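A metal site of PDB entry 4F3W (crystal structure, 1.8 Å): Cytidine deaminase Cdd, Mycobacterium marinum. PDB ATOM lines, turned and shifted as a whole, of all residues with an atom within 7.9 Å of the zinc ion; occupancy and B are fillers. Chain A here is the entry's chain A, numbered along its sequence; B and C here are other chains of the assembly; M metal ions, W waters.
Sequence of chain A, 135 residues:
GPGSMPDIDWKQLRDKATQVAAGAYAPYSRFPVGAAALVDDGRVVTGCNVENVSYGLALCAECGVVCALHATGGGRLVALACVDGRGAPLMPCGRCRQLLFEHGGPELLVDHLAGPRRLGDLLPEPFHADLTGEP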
ATOM      1  N   ALA A  58      15.347  18.419 -31.728  1.00  0.00           N
ATOM      2  CA  ALA A  58      15.585  18.449 -30.263  1.00  0.00           C
ATOM      3  C   ALA A  58      14.659  19.453 -29.606  1.00  0.00           C
ATOM      4  O   ALA A  58      14.323  20.484 -30.205  1.00  0.00           O
ATOM      5  CB  ALA A  58      17.034  18.826 -29.976  1.00  0.00           C
ATOM      6  N   LEU A  59      14.180  19.128 -28.405  1.00  0.00           N
ATOM      7  CA  LEU A  59      13.256  19.950 -27.611  1.00  0.00           C
ATOM      8  C   LEU A  59      14.011  20.450 -26.406  1.00  0.00           C
ATOM      9  O   LEU A  59      14.659  19.667 -25.736  1.00  0.00           O
ATOM     10  CB  LEU A  59      12.046  19.105 -27.183  1.00  0.00           C
ATOM     11  CG  LEU A  59      11.085  18.689 -28.340  1.00  0.00           C
ATOM     12  CD1 LEU A  59      10.172  17.516 -27.964  1.00  0.00           C
ATOM     13  CD2 LEU A  59      10.245  19.878 -28.769  1.00  0.00           C
ATOM     14  N   CYS A  60      13.944  21.753 -26.137  1.00  0.00           N
ATOM     15  CA  CYS A  60      14.611  22.339 -24.994  1.00  0.00           C
ATOM     16  C   CYS A  60      13.742  22.061 -23.769  1.00  0.00           C
ATOM     17  O   CYS A  60      12.583  21.784 -23.903  1.00  0.00           O
ATOM     18  CB  CYS A  60      14.804  23.857 -25.182  1.00  0.00           C
ATOM     19  SG  CYS A  60      15.990  24.361 -26.467  1.00  0.00           S
ATOM     20  N   ALA A  61      14.322  22.164 -22.581  1.00  0.00           N
ATOM     21  CA  ALA A  61      13.565  22.037 -21.323  1.00  0.00           C
ATOM     22  C   ALA A  61      12.396  22.998 -21.320  1.00  0.00           C
ATOM     23  O   ALA A  61      11.294  22.645 -20.930  1.00  0.00           O
ATOM     24  CB  ALA A  61      14.463  22.343 -20.103  1.00  0.00           C
ATOM     25  N   GLU A  62      12.648  24.211 -21.812  1.00  0.00           N
ATOM     26  CA  GLU A  62      11.583  25.229 -21.838  1.00  0.00           C
ATOM     27  C   GLU A  62      10.417  24.887 -22.773  1.00  0.00           C
ATOM     28  O   GLU A  62       9.296  25.315 -22.500  1.00  0.00           O
ATOM     29  CB  GLU A  62      12.159  26.616 -22.187  1.00  0.00           C
ATOM     30  CG  GLU A  62      13.311  27.030 -21.300  1.00  0.00           C
ATOM     31  CD  GLU A  62      14.669  26.689 -21.919  1.00  0.00           C
ATOM     32  OE1 GLU A  62      14.967  25.522 -22.247  1.00  0.00           O
ATOM     33  OE2 GLU A  62      15.437  27.615 -22.059  1.00  0.00           O
ATOM     34  N   CYS A  63      10.659  24.100 -23.811  1.00  0.00           N
ATOM     35  CA  CYS A  63       9.553  23.584 -24.671  1.00  0.00           C
ATOM     36  C   CYS A  63       8.678  22.662 -23.832  1.00  0.00           C
ATOM     37  O   CYS A  63       7.478  22.643 -23.951  1.00  0.00           O
ATOM     38  CB  CYS A  63      10.081  22.782 -25.863  1.00  0.00           C
ATOM     39  SG  CYS A  63      11.093  23.721 -27.047  1.00  0.00           S
ATOM     40  N   MET A  91      20.440  30.792 -19.331  1.00  0.00           N
ATOM     41  CA  MET A  91      19.582  31.712 -20.081  1.00  0.00           C
ATOM     42  C   MET A  91      18.966  30.909 -21.238  1.00  0.00           C
ATOM     43  O   MET A  91      19.664  30.190 -21.926  1.00  0.00           O
ATOM     44  CB  MET A  91      20.386  32.901 -20.624  1.00  0.00           C
ATOM     45  CG  MET A  91      20.720  33.985 -19.592  1.00  0.00           C
ATOM     46  SD  MET A  91      19.336  34.678 -18.631  1.00  0.00           S
ATOM     47  CE  MET A  91      19.413  33.508 -17.238  1.00  0.00           C
ATOM     48  N   PRO A  92      17.649  31.006 -21.432  1.00  0.00           N
ATOM     49  CA  PRO A  92      16.993  30.377 -22.560  1.00  0.00           C
ATOM     50  C   PRO A  92      17.598  30.794 -23.899  1.00  0.00           C
ATOM     51  O   PRO A  92      17.926  31.943 -24.049  1.00  0.00           O
ATOM     52  CB  PRO A  92      15.573  30.913 -22.455  1.00  0.00           C
ATOM     53  CG  PRO A  92      15.368  31.024 -20.980  1.00  0.00           C
ATOM     54  CD  PRO A  92      16.676  31.555 -20.479  1.00  0.00           C
ATOM     55  N   CYS A  93      17.611  29.892 -24.871  1.00  0.00           N
ATOM     56  CA  CYS A  93      18.027  30.214 -26.230  1.00  0.00           C
ATOM     57  C   CYS A  93      16.986  31.087 -26.828  1.00  0.00           C
ATOM     58  O   CYS A  93      15.894  31.252 -26.287  1.00  0.00           O
ATOM     59  CB  CYS A  93      18.248  28.960 -27.096  1.00  0.00           C
ATOM     60  SG  CYS A  93      16.749  28.124 -27.711  1.00  0.00           S
ATOM     61  N   GLY A  94      17.309  31.698 -27.953  1.00  0.00           N
ATOM     62  CA  GLY A  94      16.387  32.637 -28.539  1.00  0.00           C
ATOM     63  C   GLY A  94      15.058  32.067 -28.901  1.00  0.00           C
ATOM     64  O   GLY A  94      14.010  32.756 -28.822  1.00  0.00           O
ATOM     65  N   ARG A  95      15.051  30.836 -29.397  1.00  0.00           N
ATOM     66  CA  ARG A  95      13.796  30.157 -29.723  1.00  0.00           C
ATOM     67  C   ARG A  95      12.929  30.097 -28.457  1.00  0.00           C
ATOM     68  O   ARG A  95      11.729  30.426 -28.436  1.00  0.00           O
ATOM     69  CB  ARG A  95      14.104  28.727 -30.256  1.00  0.00           C
ATOM     70  CG  ARG A  95      12.921  27.873 -30.668  1.00  0.00           C
ATOM     71  CD  ARG A  95      12.399  27.013 -29.499  1.00  0.00           C
ATOM     72  NE  ARG A  95      13.290  25.907 -29.127  1.00  0.00           N
ATOM     73  CZ  ARG A  95      13.343  24.711 -29.734  1.00  0.00           C
ATOM     74  NH1 ARG A  95      12.560  24.444 -30.782  1.00  0.00           N
ATOM     75  NH2 ARG A  95      14.168  23.766 -29.295  1.00  0.00           N
ATOM     76  N   CYS A  96      13.560  29.708 -27.356  1.00  0.00           N
ATOM     77  CA  CYS A  96      12.827  29.568 -26.111  1.00  0.00           C
ATOM     78  C   CYS A  96      12.394  30.921 -25.569  1.00  0.00           C
ATOM     79  O   CYS A  96      11.323  31.010 -24.984  1.00  0.00           O
ATOM     80  CB  CYS A  96      13.623  28.750 -25.114  1.00  0.00           C
ATOM     81  SG  CYS A  96      13.597  27.025 -25.617  1.00  0.00           S
ATOM     82  N   ARG A  97      13.187  31.972 -25.788  1.00  0.00           N
ATOM     83  CA  ARG A  97      12.727  33.312 -25.398  1.00  0.00           C
ATOM     84  C   ARG A  97      11.416  33.679 -26.104  1.00  0.00           C
ATOM     85  O   ARG A  97      10.514  34.285 -25.493  1.00  0.00           O
ATOM     86  CB  ARG A  97      13.789  34.355 -25.648  1.00  0.00           C
ATOM     87  CG  ARG A  97      15.013  34.150 -24.777  1.00  0.00           C
ATOM     88  CD  ARG A  97      16.091  35.157 -25.101  1.00  0.00           C
ATOM     89  NE  ARG A  97      17.365  34.690 -24.549  1.00  0.00           N
ATOM     90  CZ  ARG A  97      18.484  35.417 -24.426  1.00  0.00           C
ATOM     91  NH1 ARG A  97      18.537  36.678 -24.796  1.00  0.00           N
ATOM     92  NH2 ARG A  97      19.543  34.847 -23.887  1.00  0.00           N
ATOM     93  N   LEU A  99       9.173  31.577 -27.397  1.00  0.00           N
ATOM     94  CA  LEU A  99       8.211  30.663 -26.769  1.00  0.00           C
ATOM     95  C   LEU A  99       7.716  31.256 -25.472  1.00  0.00           C
ATOM     96  O   LEU A  99       6.520  31.380 -25.242  1.00  0.00           O
ATOM     97  CB  LEU A  99       8.862  29.291 -26.502  1.00  0.00           C
ATOM     98  CG  LEU A  99       8.891  28.241 -27.598  1.00  0.00           C
ATOM     99  CD1 LEU A  99       9.276  26.872 -26.988  1.00  0.00           C
ATOM    100  CD2 LEU A  99       7.542  28.111 -28.294  1.00  0.00           C
ATOM    101  N   LEU A 100       8.642  31.608 -24.591  1.00  0.00           N
ATOM    102  CA  LEU A 100       8.221  32.082 -23.272  1.00  0.00           C
ATOM    103  C   LEU A 100       7.451  33.385 -23.341  1.00  0.00           C
ATOM    104  O   LEU A 100       6.551  33.656 -22.509  1.00  0.00           O
ATOM    105  CB  LEU A 100       9.444  32.192 -22.370  1.00  0.00           C
ATOM    106  CG  LEU A 100      10.014  30.808 -22.077  1.00  0.00           C
ATOM    107  CD1 LEU A 100      11.454  30.955 -21.599  1.00  0.00           C
ATOM    108  CD2 LEU A 100       9.114  30.100 -21.033  1.00  0.00           C
ATOM    109  N   SER B  54      22.206  25.681 -30.174  1.00  0.00           N
ATOM    110  CA  SER B  54      20.924  25.173 -29.728  1.00  0.00           C
ATOM    111  C   SER B  54      20.505  24.113 -30.732  1.00  0.00           C
ATOM    112  O   SER B  54      20.067  24.433 -31.849  1.00  0.00           O
ATOM    113  CB  SER B  54      19.880  26.296 -29.658  1.00  0.00           C
ATOM    114  OG  SER B  54      18.704  25.794 -29.025  1.00  0.00           O
ATOM    115  N   TYR B  55      20.656  22.834 -30.363  1.00  0.00           N
ATOM    116  CA  TYR B  55      20.541  21.781 -31.396  1.00  0.00           C
ATOM    117  C   TYR B  55      19.245  21.806 -32.171  1.00  0.00           C
ATOM    118  O   TYR B  55      19.233  21.525 -33.390  1.00  0.00           O
ATOM    119  CB  TYR B  55      20.676  20.398 -30.768  1.00  0.00           C
ATOM    120  CG  TYR B  55      22.085  19.949 -30.471  1.00  0.00           C
ATOM    121  CD1 TYR B  55      23.157  20.854 -30.404  1.00  0.00           C
ATOM    122  CD2 TYR B  55      22.333  18.613 -30.213  1.00  0.00           C
ATOM    123  CE1 TYR B  55      24.454  20.402 -30.100  1.00  0.00           C
ATOM    124  CE2 TYR B  55      23.602  18.166 -29.898  1.00  0.00           C
ATOM    125  CZ  TYR B  55      24.651  19.051 -29.852  1.00  0.00           C
ATOM    126  OH  TYR B  55      25.899  18.560 -29.555  1.00  0.00           O
ATOM    127  N   GLY B  56      18.155  22.115 -31.469  1.00  0.00           N
ATOM    128  CA  GLY B  56      16.834  22.135 -32.079  1.00  0.00           C
ATOM    129  C   GLY B  56      16.604  23.206 -33.149  1.00  0.00           C
ATOM    130  O   GLY B  56      15.512  23.251 -33.755  1.00  0.00           O
ATOM    131  N   LEU B  57      17.621  24.040 -33.388  1.00  0.00           N
ATOM    132  CA  LEU B  57      17.540  25.040 -34.436  1.00  0.00           C
ATOM    133  C   LEU B  57      18.236  24.605 -35.708  1.00  0.00           C
ATOM    134  O   LEU B  57      18.220  25.334 -36.692  1.00  0.00           O
ATOM    135  CB  LEU B  57      18.137  26.370 -33.929  1.00  0.00           C
ATOM    136  CG  LEU B  57      17.439  26.837 -32.623  1.00  0.00           C
ATOM    137  CD1 LEU B  57      17.730  28.327 -32.487  1.00  0.00           C
ATOM    138  CD2 LEU B  57      15.947  26.579 -32.506  1.00  0.00           C
ATOM    139  N   GLN C  98      18.751  33.703 -32.615  1.00  0.00           N
ATOM    140  CA  GLN C  98      19.751  32.672 -32.257  1.00  0.00           C
ATOM    141  C   GLN C  98      20.477  32.107 -33.484  1.00  0.00           C
ATOM    142  O   GLN C  98      21.695  31.828 -33.428  1.00  0.00           O
ATOM    143  CB  GLN C  98      19.069  31.550 -31.512  1.00  0.00           C
ATOM    144  CG  GLN C  98      20.051  30.565 -30.863  1.00  0.00           C
ATOM    145  CD  GLN C  98      20.735  31.131 -29.644  1.00  0.00           C
ATOM    146  OE1 GLN C  98      20.108  31.585 -28.681  1.00  0.00           O
ATOM    147  NE2 GLN C  98      22.072  31.070 -29.657  1.00  0.00           N
HETATM  148 ZN    ZN M   1      15.881  26.657 -26.111  1.00  0.00          ZN
HETATM  149  O   HOH W   1      16.873  27.078 -24.371  1.00  0.00           O
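The side-chain sulfur (SG) of Cys 60 sits close to the guanidinium group (NH2) of Arg 95, 3.4 Å away. N of Cys 60 lies within hydrogen-bond range of SG of Cys 63 (3.6 Å). SG of Cys 93 lies close to N of Arg 95, 3.6 Å away. The side-chain sulfur (SG) of Cys 93 lies close to the side-chain hydroxyl (OG) of Ser 54 of chain B. SG of Cys 96 lies close to NE of Arg 95 (3.7 Å).
Of the 20 residues printed, 3 come within 4 Å of the zinc ion. The nearest printed residue that does not touch the zinc ion is Arg 95 (4.05 Å).
Water W1 is bound to the zinc ion, 2.0 Å away. The side-chain sulfur (SG) of Cys 60 binds the zinc ion (2.3 Å). The side-chain sulfur (SG) of Cys 93 binds the zinc ion. The zinc ion is bound by the side-chain sulfur (SG) of Cys 96, 2.4 Å away. The zinc ion has four donor atoms within binding distance.
Water W1 lies within hydrogen-bond range of OE2 of Glu 62 (2.8 Å) and N of Cys 93 (3.0 Å).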
